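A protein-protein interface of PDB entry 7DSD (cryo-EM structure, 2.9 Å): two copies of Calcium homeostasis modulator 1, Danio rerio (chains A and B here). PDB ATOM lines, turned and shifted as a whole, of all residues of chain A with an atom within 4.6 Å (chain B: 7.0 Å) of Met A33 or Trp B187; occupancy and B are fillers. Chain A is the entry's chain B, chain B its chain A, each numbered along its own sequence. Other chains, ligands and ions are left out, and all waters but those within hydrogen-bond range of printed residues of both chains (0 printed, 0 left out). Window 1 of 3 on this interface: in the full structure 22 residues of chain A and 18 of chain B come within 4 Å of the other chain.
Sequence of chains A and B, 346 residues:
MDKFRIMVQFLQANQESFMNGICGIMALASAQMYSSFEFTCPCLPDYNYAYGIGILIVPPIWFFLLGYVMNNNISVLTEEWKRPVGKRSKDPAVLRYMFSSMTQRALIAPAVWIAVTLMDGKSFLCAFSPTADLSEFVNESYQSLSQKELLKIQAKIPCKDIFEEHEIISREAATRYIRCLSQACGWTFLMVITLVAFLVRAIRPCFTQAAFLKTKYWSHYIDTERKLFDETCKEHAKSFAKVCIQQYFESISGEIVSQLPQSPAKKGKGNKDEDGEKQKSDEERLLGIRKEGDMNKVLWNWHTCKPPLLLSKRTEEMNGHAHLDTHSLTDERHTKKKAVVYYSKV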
ATOM      1  N   ALA A  29       1.916   9.448  14.037  1.00  0.00           N
ATOM      2  CA  ALA A  29       2.922   8.785  13.213  1.00  0.00           C
ATOM      3  C   ALA A  29       2.696   7.280  13.183  1.00  0.00           C
ATOM      4  O   ALA A  29       2.670   6.666  12.112  1.00  0.00           O
ATOM      5  CB  ALA A  29       4.322   9.113  13.729  1.00  0.00           C
ATOM      6  N   SER A  30       2.513   6.670  14.355  1.00  0.00           N
ATOM      7  CA  SER A  30       2.297   5.229  14.418  1.00  0.00           C
ATOM      8  C   SER A  30       0.970   4.841  13.778  1.00  0.00           C
ATOM      9  O   SER A  30       0.878   3.831  13.067  1.00  0.00           O
ATOM     10  CB  SER A  30       2.354   4.758  15.868  1.00  0.00           C
ATOM     11  OG  SER A  30       1.373   5.418  16.641  1.00  0.00           O
ATOM     12  N   ALA A  31      -0.077   5.631  14.026  1.00  0.00           N
ATOM     13  CA  ALA A  31      -1.373   5.341  13.420  1.00  0.00           C
ATOM     14  C   ALA A  31      -1.281   5.360  11.898  1.00  0.00           C
ATOM     15  O   ALA A  31      -1.751   4.437  11.220  1.00  0.00           O
ATOM     16  CB  ALA A  31      -2.416   6.343  13.910  1.00  0.00           C
ATOM     17  N   GLN A  32      -0.664   6.405  11.342  1.00  0.00           N
ATOM     18  CA  GLN A  32      -0.530   6.508   9.896  1.00  0.00           C
ATOM     19  C   GLN A  32       0.366   5.411   9.342  1.00  0.00           C
ATOM     20  O   GLN A  32       0.117   4.892   8.247  1.00  0.00           O
ATOM     21  CB  GLN A  32       0.015   7.887   9.524  1.00  0.00           C
ATOM     22  CG  GLN A  32       0.011   8.175   8.038  1.00  0.00           C
ATOM     23  CD  GLN A  32      -1.387   8.357   7.482  1.00  0.00           C
ATOM     24  OE1 GLN A  32      -2.353   8.501   8.231  1.00  0.00           O
ATOM     25  NE2 GLN A  32      -1.500   8.352   6.158  1.00  0.00           N
ATOM     26  N   MET A  33       1.416   5.044  10.080  1.00  0.00           N
ATOM     27  CA  MET A  33       2.288   3.969   9.622  1.00  0.00           C
ATOM     28  C   MET A  33       1.533   2.653   9.539  1.00  0.00           C
ATOM     29  O   MET A  33       1.736   1.872   8.603  1.00  0.00           O
ATOM     30  CB  MET A  33       3.496   3.835  10.544  1.00  0.00           C
ATOM     31  CG  MET A  33       4.456   2.743  10.124  1.00  0.00           C
ATOM     32  SD  MET A  33       5.926   2.664  11.155  1.00  0.00           S
ATOM     33  CE  MET A  33       6.813   1.329  10.357  1.00  0.00           C
ATOM     34  N   TYR A  34       0.654   2.385  10.506  1.00  0.00           N
ATOM     35  CA  TYR A  34      -0.184   1.196  10.397  1.00  0.00           C
ATOM     36  C   TYR A  34      -1.132   1.311   9.212  1.00  0.00           C
ATOM     37  O   TYR A  34      -1.374   0.330   8.502  1.00  0.00           O
ATOM     38  CB  TYR A  34      -0.977   0.956  11.679  1.00  0.00           C
ATOM     39  CG  TYR A  34      -1.794  -0.315  11.615  1.00  0.00           C
ATOM     40  CD1 TYR A  34      -1.248  -1.532  11.991  1.00  0.00           C
ATOM     41  CD2 TYR A  34      -3.103  -0.305  11.157  1.00  0.00           C
ATOM     42  CE1 TYR A  34      -1.982  -2.696  11.924  1.00  0.00           C
ATOM     43  CE2 TYR A  34      -3.845  -1.464  11.086  1.00  0.00           C
ATOM     44  CZ  TYR A  34      -3.279  -2.657  11.472  1.00  0.00           C
ATOM     45  OH  TYR A  34      -4.014  -3.815  11.406  1.00  0.00           O
ATOM     46  N   SER A  35      -1.691   2.505   8.995  1.00  0.00           N
ATOM     47  CA  SER A  35      -2.623   2.680   7.887  1.00  0.00           C
ATOM     48  C   SER A  35      -1.963   2.397   6.544  1.00  0.00           C
ATOM     49  O   SER A  35      -2.612   1.871   5.633  1.00  0.00           O
ATOM     50  CB  SER A  35      -3.202   4.094   7.907  1.00  0.00           C
ATOM     51  OG  SER A  35      -3.882   4.347   9.122  1.00  0.00           O
ATOM     52  N   SER A  36      -0.680   2.729   6.404  1.00  0.00           N
ATOM     53  CA  SER A  36       0.060   2.534   5.164  1.00  0.00           C
ATOM     54  C   SER A  36       0.985   1.322   5.223  1.00  0.00           C
ATOM     55  O   SER A  36       2.050   1.324   4.600  1.00  0.00           O
ATOM     56  CB  SER A  36       0.859   3.790   4.825  1.00  0.00           C
ATOM     57  OG  SER A  36       1.829   4.053   5.823  1.00  0.00           O
ATOM     58  N   PHE A  37       0.597   0.288   5.959  1.00  0.00           N
ATOM     59  CA  PHE A  37       1.386  -0.927   6.096  1.00  0.00           C
ATOM     60  C   PHE A  37       0.618  -2.084   5.480  1.00  0.00           C
ATOM     61  O   PHE A  37      -0.559  -2.289   5.791  1.00  0.00           O
ATOM     62  CB  PHE A  37       1.702  -1.215   7.563  1.00  0.00           C
ATOM     63  CG  PHE A  37       2.387  -2.526   7.790  1.00  0.00           C
ATOM     64  CD1 PHE A  37       3.729  -2.677   7.506  1.00  0.00           C
ATOM     65  CD2 PHE A  37       1.691  -3.606   8.297  1.00  0.00           C
ATOM     66  CE1 PHE A  37       4.359  -3.882   7.716  1.00  0.00           C
ATOM     67  CE2 PHE A  37       2.317  -4.812   8.508  1.00  0.00           C
ATOM     68  CZ  PHE A  37       3.655  -4.950   8.218  1.00  0.00           C
ATOM     69  N   ILE A  55       3.764  -8.968  14.341  1.00  0.00           N
ATOM     70  CA  ILE A  55       3.177  -7.679  13.994  1.00  0.00           C
ATOM     71  C   ILE A  55       2.561  -7.027  15.222  1.00  0.00           C
ATOM     72  O   ILE A  55       2.549  -5.795  15.344  1.00  0.00           O
ATOM     73  CB  ILE A  55       2.149  -7.850  12.859  1.00  0.00           C
ATOM     74  CG1 ILE A  55       2.867  -8.200  11.563  1.00  0.00           C
ATOM     75  CG2 ILE A  55       1.349  -6.585  12.657  1.00  0.00           C
ATOM     76  CD1 ILE A  55       3.832  -7.139  11.118  1.00  0.00           C
ATOM     77  N   PRO A  59       6.657  -3.884  16.456  1.00  0.00           N
ATOM     78  CA  PRO A  59       6.590  -2.450  16.156  1.00  0.00           C
ATOM     79  C   PRO A  59       6.408  -1.588  17.396  1.00  0.00           C
ATOM     80  O   PRO A  59       6.983  -0.494  17.460  1.00  0.00           O
ATOM     81  CB  PRO A  59       5.387  -2.345  15.213  1.00  0.00           C
ATOM     82  CG  PRO A  59       5.370  -3.636  14.532  1.00  0.00           C
ATOM     83  CD  PRO A  59       5.756  -4.641  15.567  1.00  0.00           C
ATOM     84  N   TRP A  62       9.815  -1.171  18.872  1.00  0.00           N
ATOM     85  CA  TRP A  62      10.615  -0.233  18.094  1.00  0.00           C
ATOM     86  C   TRP A  62      10.183   1.205  18.346  1.00  0.00           C
ATOM     87  O   TRP A  62      11.023   2.105  18.425  1.00  0.00           O
ATOM     88  CB  TRP A  62      10.532  -0.557  16.607  1.00  0.00           C
ATOM     89  CG  TRP A  62      11.211   0.472  15.776  1.00  0.00           C
ATOM     90  CD1 TRP A  62      12.539   0.760  15.764  1.00  0.00           C
ATOM     91  CD2 TRP A  62      10.598   1.365  14.846  1.00  0.00           C
ATOM     92  NE1 TRP A  62      12.797   1.776  14.880  1.00  0.00           N
ATOM     93  CE2 TRP A  62      11.618   2.165  14.302  1.00  0.00           C
ATOM     94  CE3 TRP A  62       9.287   1.564  14.415  1.00  0.00           C
ATOM     95  CZ2 TRP A  62      11.368   3.146  13.353  1.00  0.00           C
ATOM     96  CZ3 TRP A  62       9.040   2.539  13.474  1.00  0.00           C
ATOM     97  CH2 TRP A  62      10.076   3.318  12.952  1.00  0.00           C
ATOM     98  N   PHE A  63       8.877   1.444  18.473  1.00  0.00           N
ATOM     99  CA  PHE A  63       8.404   2.796  18.755  1.00  0.00           C
ATOM    100  C   PHE A  63       8.845   3.251  20.137  1.00  0.00           C
ATOM    101  O   PHE A  63       9.144   4.431  20.343  1.00  0.00           O
ATOM    102  CB  PHE A  63       6.884   2.871  18.638  1.00  0.00           C
ATOM    103  CG  PHE A  63       6.388   2.989  17.229  1.00  0.00           C
ATOM    104  CD1 PHE A  63       6.702   4.091  16.462  1.00  0.00           C
ATOM    105  CD2 PHE A  63       5.584   2.009  16.683  1.00  0.00           C
ATOM    106  CE1 PHE A  63       6.240   4.199  15.169  1.00  0.00           C
ATOM    107  CE2 PHE A  63       5.124   2.112  15.395  1.00  0.00           C
ATOM    108  CZ  PHE A  63       5.449   3.208  14.636  1.00  0.00           C
ATOM    109  N   TRP A 113      -0.325   1.992  18.720  1.00  0.00           N
ATOM    110  CA  TRP A 113      -0.150   0.924  17.743  1.00  0.00           C
ATOM    111  C   TRP A 113      -0.939  -0.315  18.139  1.00  0.00           C
ATOM    112  O   TRP A 113      -1.617  -0.924  17.304  1.00  0.00           O
ATOM    113  CB  TRP A 113       1.330   0.580  17.578  1.00  0.00           C
ATOM    114  CG  TRP A 113       1.551  -0.621  16.708  1.00  0.00           C
ATOM    115  CD1 TRP A 113       1.564  -1.923  17.103  1.00  0.00           C
ATOM    116  CD2 TRP A 113       1.785  -0.629  15.297  1.00  0.00           C
ATOM    117  NE1 TRP A 113       1.791  -2.742  16.030  1.00  0.00           N
ATOM    118  CE2 TRP A 113       1.933  -1.972  14.909  1.00  0.00           C
ATOM    119  CE3 TRP A 113       1.887   0.367  14.326  1.00  0.00           C
ATOM    120  CZ2 TRP A 113       2.175  -2.342  13.593  1.00  0.00           C
ATOM    121  CZ3 TRP A 113       2.129  -0.004  13.022  1.00  0.00           C
ATOM    122  CH2 TRP A 113       2.269  -1.346  12.667  1.00  0.00           C
ATOM    123  N   PHE B  10       0.810   9.466   4.104  1.00  0.00           N
ATOM    124  CA  PHE B  10       1.775   9.448   5.198  1.00  0.00           C
ATOM    125  C   PHE B  10       2.788  10.577   5.058  1.00  0.00           C
ATOM    126  O   PHE B  10       3.183  11.193   6.054  1.00  0.00           O
ATOM    127  CB  PHE B  10       2.484   8.094   5.251  1.00  0.00           C
ATOM    128  N   ALA B 115      14.488   0.857   4.371  1.00  0.00           N
ATOM    129  CA  ALA B 115      13.385   0.389   5.202  1.00  0.00           C
ATOM    130  C   ALA B 115      12.095   0.302   4.401  1.00  0.00           C
ATOM    131  O   ALA B 115      11.388  -0.709   4.451  1.00  0.00           O
ATOM    132  CB  ALA B 115      13.211   1.309   6.407  1.00  0.00           C
ATOM    133  N   LEU B 118      12.096  -2.489   1.924  1.00  0.00           N
ATOM    134  CA  LEU B 118      12.034  -3.806   2.542  1.00  0.00           C
ATOM    135  C   LEU B 118      10.644  -4.125   3.077  1.00  0.00           C
ATOM    136  O   LEU B 118      10.194  -5.269   2.967  1.00  0.00           O
ATOM    137  CB  LEU B 118      13.060  -3.908   3.671  1.00  0.00           C
ATOM    138  CG  LEU B 118      14.492  -4.210   3.238  1.00  0.00           C
ATOM    139  CD1 LEU B 118      15.423  -4.173   4.428  1.00  0.00           C
ATOM    140  CD2 LEU B 118      14.550  -5.557   2.555  1.00  0.00           C
ATOM    141  N   MET B 119       9.953  -3.138   3.654  1.00  0.00           N
ATOM    142  CA  MET B 119       8.611  -3.396   4.165  1.00  0.00           C
ATOM    143  C   MET B 119       7.650  -3.777   3.049  1.00  0.00           C
ATOM    144  O   MET B 119       6.726  -4.565   3.270  1.00  0.00           O
ATOM    145  CB  MET B 119       8.082  -2.180   4.922  1.00  0.00           C
ATOM    146  CG  MET B 119       8.956  -1.726   6.075  1.00  0.00           C
ATOM    147  SD  MET B 119       9.406  -3.059   7.192  1.00  0.00           S
ATOM    148  CE  MET B 119       7.786  -3.599   7.703  1.00  0.00           C
ATOM    149  N   LEU B 181       8.810 -12.901   4.448  1.00  0.00           N
ATOM    150  CA  LEU B 181      10.255 -12.911   4.676  1.00  0.00           C
ATOM    151  C   LEU B 181      10.842 -11.508   4.558  1.00  0.00           C
ATOM    152  O   LEU B 181      11.648 -11.079   5.398  1.00  0.00           O
ATOM    153  CB  LEU B 181      10.936 -13.859   3.694  1.00  0.00           C
ATOM    154  CG  LEU B 181      11.437 -15.169   4.291  1.00  0.00           C
ATOM    155  CD1 LEU B 181      10.313 -15.883   5.009  1.00  0.00           C
ATOM    156  CD2 LEU B 181      12.023 -16.047   3.206  1.00  0.00           C
ATOM    157  N   SER B 182      10.445 -10.778   3.515  1.00  0.00           N
ATOM    158  CA  SER B 182      10.973  -9.435   3.309  1.00  0.00           C
ATOM    159  C   SER B 182      10.601  -8.506   4.457  1.00  0.00           C
ATOM    160  O   SER B 182      11.418  -7.689   4.893  1.00  0.00           O
ATOM    161  CB  SER B 182      10.467  -8.872   1.987  1.00  0.00           C
ATOM    162  OG  SER B 182      10.868  -7.524   1.830  1.00  0.00           O
ATOM    163  N   GLN B 183       9.367  -8.609   4.954  1.00  0.00           N
ATOM    164  CA  GLN B 183       8.954  -7.740   6.053  1.00  0.00           C
ATOM    165  C   GLN B 183       9.704  -8.076   7.337  1.00  0.00           C
ATOM    166  O   GLN B 183      10.056  -7.177   8.110  1.00  0.00           O
ATOM    167  CB  GLN B 183       7.447  -7.838   6.265  1.00  0.00           C
ATOM    168  CG  GLN B 183       6.651  -7.272   5.114  1.00  0.00           C
ATOM    169  CD  GLN B 183       5.180  -7.177   5.416  1.00  0.00           C
ATOM    170  OE1 GLN B 183       4.723  -7.608   6.472  1.00  0.00           O
ATOM    171  NE2 GLN B 183       4.425  -6.605   4.489  1.00  0.00           N
ATOM    172  N   ALA B 184       9.954  -9.362   7.584  1.00  0.00           N
ATOM    173  CA  ALA B 184      10.772  -9.740   8.732  1.00  0.00           C
ATOM    174  C   ALA B 184      12.157  -9.116   8.641  1.00  0.00           C
ATOM    175  O   ALA B 184      12.680  -8.570   9.624  1.00  0.00           O
ATOM    176  CB  ALA B 184      10.873 -11.261   8.827  1.00  0.00           C
ATOM    177  N   CYS B 185      12.773  -9.199   7.459  1.00  0.00           N
ATOM    178  CA  CYS B 185      14.087  -8.588   7.274  1.00  0.00           C
ATOM    179  C   CYS B 185      14.034  -7.082   7.502  1.00  0.00           C
ATOM    180  O   CYS B 185      14.933  -6.512   8.131  1.00  0.00           O
ATOM    181  CB  CYS B 185      14.626  -8.902   5.882  1.00  0.00           C
ATOM    182  SG  CYS B 185      15.040 -10.637   5.627  1.00  0.00           S
ATOM    183  N   GLY B 186      12.993  -6.423   6.996  1.00  0.00           N
ATOM    184  CA  GLY B 186      12.876  -4.988   7.192  1.00  0.00           C
ATOM    185  C   GLY B 186      12.748  -4.607   8.656  1.00  0.00           C
ATOM    186  O   GLY B 186      13.332  -3.616   9.105  1.00  0.00           O
ATOM    187  N   TRP B 187      12.001  -5.399   9.423  1.00  0.00           N
ATOM    188  CA  TRP B 187      11.854  -5.094  10.842  1.00  0.00           C
ATOM    189  C   TRP B 187      13.159  -5.313  11.594  1.00  0.00           C
ATOM    190  O   TRP B 187      13.514  -4.519  12.475  1.00  0.00           O
ATOM    191  CB  TRP B 187      10.727  -5.922  11.453  1.00  0.00           C
ATOM    192  CG  TRP B 187       9.379  -5.328  11.217  1.00  0.00           C
ATOM    193  CD1 TRP B 187       8.333  -5.906  10.570  1.00  0.00           C
ATOM    194  CD2 TRP B 187       8.937  -4.025  11.611  1.00  0.00           C
ATOM    195  NE1 TRP B 187       7.260  -5.051  10.546  1.00  0.00           N
ATOM    196  CE2 TRP B 187       7.608  -3.888  11.177  1.00  0.00           C
ATOM    197  CE3 TRP B 187       9.533  -2.963  12.296  1.00  0.00           C
ATOM    198  CZ2 TRP B 187       6.866  -2.734  11.399  1.00  0.00           C
ATOM    199  CZ3 TRP B 187       8.796  -1.821  12.515  1.00  0.00           C
ATOM    200  CH2 TRP B 187       7.477  -1.714  12.069  1.00  0.00           C
ATOM    201  N   THR B 188      13.894  -6.378  11.263  1.00  0.00           N
ATOM    202  CA  THR B 188      15.202  -6.565  11.888  1.00  0.00           C
ATOM    203  C   THR B 188      16.136  -5.408  11.561  1.00  0.00           C
ATOM    204  O   THR B 188      16.879  -4.931  12.429  1.00  0.00           O
ATOM    205  CB  THR B 188      15.822  -7.886  11.444  1.00  0.00           C
ATOM    206  OG1 THR B 188      15.870  -7.938  10.016  1.00  0.00           O
ATOM    207  CG2 THR B 188      15.007  -9.050  11.958  1.00  0.00           C
ATOM    208  N   PHE B 189      16.105  -4.938  10.312  1.00  0.00           N
ATOM    209  CA  PHE B 189      16.923  -3.794   9.925  1.00  0.00           C
ATOM    210  C   PHE B 189      16.569  -2.565  10.752  1.00  0.00           C
ATOM    211  O   PHE B 189      17.456  -1.881  11.280  1.00  0.00           O
ATOM    212  CB  PHE B 189      16.754  -3.513   8.434  1.00  0.00           C
ATOM    213  CG  PHE B 189      17.360  -2.218   7.985  1.00  0.00           C
ATOM    214  CD1 PHE B 189      18.725  -2.101   7.805  1.00  0.00           C
ATOM    215  CD2 PHE B 189      16.560  -1.124   7.724  1.00  0.00           C
ATOM    216  CE1 PHE B 189      19.279  -0.911   7.389  1.00  0.00           C
ATOM    217  CE2 PHE B 189      17.111   0.067   7.309  1.00  0.00           C
ATOM    218  CZ  PHE B 189      18.471   0.173   7.139  1.00  0.00           C
ATOM    219  N   LEU B 190      15.274  -2.260  10.864  1.00  0.00           N
ATOM    220  CA  LEU B 190      14.855  -1.097  11.643  1.00  0.00           C
ATOM    221  C   LEU B 190      15.300  -1.209  13.094  1.00  0.00           C
ATOM    222  O   LEU B 190      15.774  -0.229  13.685  1.00  0.00           O
ATOM    223  CB  LEU B 190      13.340  -0.924  11.565  1.00  0.00           C
ATOM    224  CG  LEU B 190      12.815  -0.169  10.348  1.00  0.00           C
ATOM    225  CD1 LEU B 190      11.305  -0.098  10.374  1.00  0.00           C
ATOM    226  CD2 LEU B 190      13.408   1.219  10.313  1.00  0.00           C
ATOM    227  N   MET B 191      15.173  -2.399  13.684  1.00  0.00           N
ATOM    228  CA  MET B 191      15.555  -2.562  15.082  1.00  0.00           C
ATOM    229  C   MET B 191      17.052  -2.357  15.278  1.00  0.00           C
ATOM    230  O   MET B 191      17.472  -1.672  16.220  1.00  0.00           O
ATOM    231  CB  MET B 191      15.129  -3.939  15.587  1.00  0.00           C
ATOM    232  CG  MET B 191      13.626  -4.132  15.642  1.00  0.00           C
ATOM    233  SD  MET B 191      12.812  -2.949  16.729  1.00  0.00           S
ATOM    234  CE  MET B 191      13.444  -3.466  18.320  1.00  0.00           C
ATOM    235  N   VAL B 192      17.872  -2.936  14.400  1.00  0.00           N
ATOM    236  CA  VAL B 192      19.318  -2.781  14.535  1.00  0.00           C
ATOM    237  C   VAL B 192      19.715  -1.318  14.368  1.00  0.00           C
ATOM    238  O   VAL B 192      20.548  -0.790  15.116  1.00  0.00           O
ATOM    239  CB  VAL B 192      20.050  -3.684  13.530  1.00  0.00           C
ATOM    240  CG1 VAL B 192      21.534  -3.425  13.580  1.00  0.00           C
ATOM    241  CG2 VAL B 192      19.759  -5.138  13.829  1.00  0.00           C
ATOM    242  N   ILE B 193      19.123  -0.642  13.380  1.00  0.00           N
ATOM    243  CA  ILE B 193      19.428   0.769  13.159  1.00  0.00           C
ATOM    244  C   ILE B 193      19.078   1.593  14.390  1.00  0.00           C
ATOM    245  O   ILE B 193      19.857   2.457  14.819  1.00  0.00           O
ATOM    246  CB  ILE B 193      18.696   1.279  11.906  1.00  0.00           C
ATOM    247  CG1 ILE B 193      19.328   0.689  10.651  1.00  0.00           C
ATOM    248  CG2 ILE B 193      18.726   2.787  11.840  1.00  0.00           C
ATOM    249  CD1 ILE B 193      20.809   0.936  10.563  1.00  0.00           C
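Trp B187 touches Met A33 (CH2 to CE, 3.6 Å). CE1 of Phe A37 touches CE of Met B119, at 3.4 Å. OE1 of Gln B183 touches CZ of Phe A37 (3.4 Å). CZ2 of Trp B187 touches CG of Pro A59 (3.6 Å). Trp A62 touches Trp B187. Leu B190 touches Trp A62 (O to NE1, 3.8 Å). Trp A62 touches Met B191 (CB to SD, 3.3 Å).
Hydrophobic or aromatic side chains of chain A within 4 Å of the printed part of chain B: Met A33, Phe A37, Pro A59 and Trp A62. Of the 17 printed residues of chain B, 6 touch a printed residue of chain A. Printed residues of chain B that touch a printed residue of chain A: Phe B10, Met B119, Gln B183, Trp B187, Leu B190 and Met B191. Hydrophobic or aromatic side chains of chain B that line the printed part of chain A: Phe B10, Met B119, Trp B187 and Met B191. Among the printed residues, 8 pairs touch across the chains. Among the printed residues, no Asp or Glu carboxylate lies within 4 Å of a Lys or Arg side-chain nitrogen of the other chain.
No position is printed for both chains.
Of chain B, only Trp B187 comes within 4 Å of Met A33. Of the printed residues of chain B, Phe A37 touches Met B119 and Gln B183. Of the printed residues of chain B, Pro A59 touches Trp B187. Of the printed residues of chain A, Met B119 touches Phe A37 (3.4 Å). Ser B182 touches none of the printed residues of chain A. Printed residues of chain A within 4 Å of Gln B183: Phe A37 (3.4 Å). Gly B186 touches none of the printed residues of chain A. Trp B187 touches three residues of chain A. Of the printed residues of chain A, Leu B190 touches Trp A62 (3.8 Å). The nearest residue of chain B that does not touch Met A33 is Leu B190 (4.7 Å). The nearest residue of chain A that does not touch Trp B187 is Ile A55 (4.1 Å).
The backbone carbonyl oxygen (O) of Met B119 lies close to the side-chain amide nitrogen (NE2) of Gln B183, 3.3 Å away. The backbone carbonyl oxygen (O) of Gln A32 lies within hydrogen-bond range of the side-chain hydroxyl (OG) of Ser A36, 3.1 Å away.
The backbone NH (N) of Phe B10 sits close to the side-chain amide nitrogen (NE2) of Gln A32 (3.3 Å).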
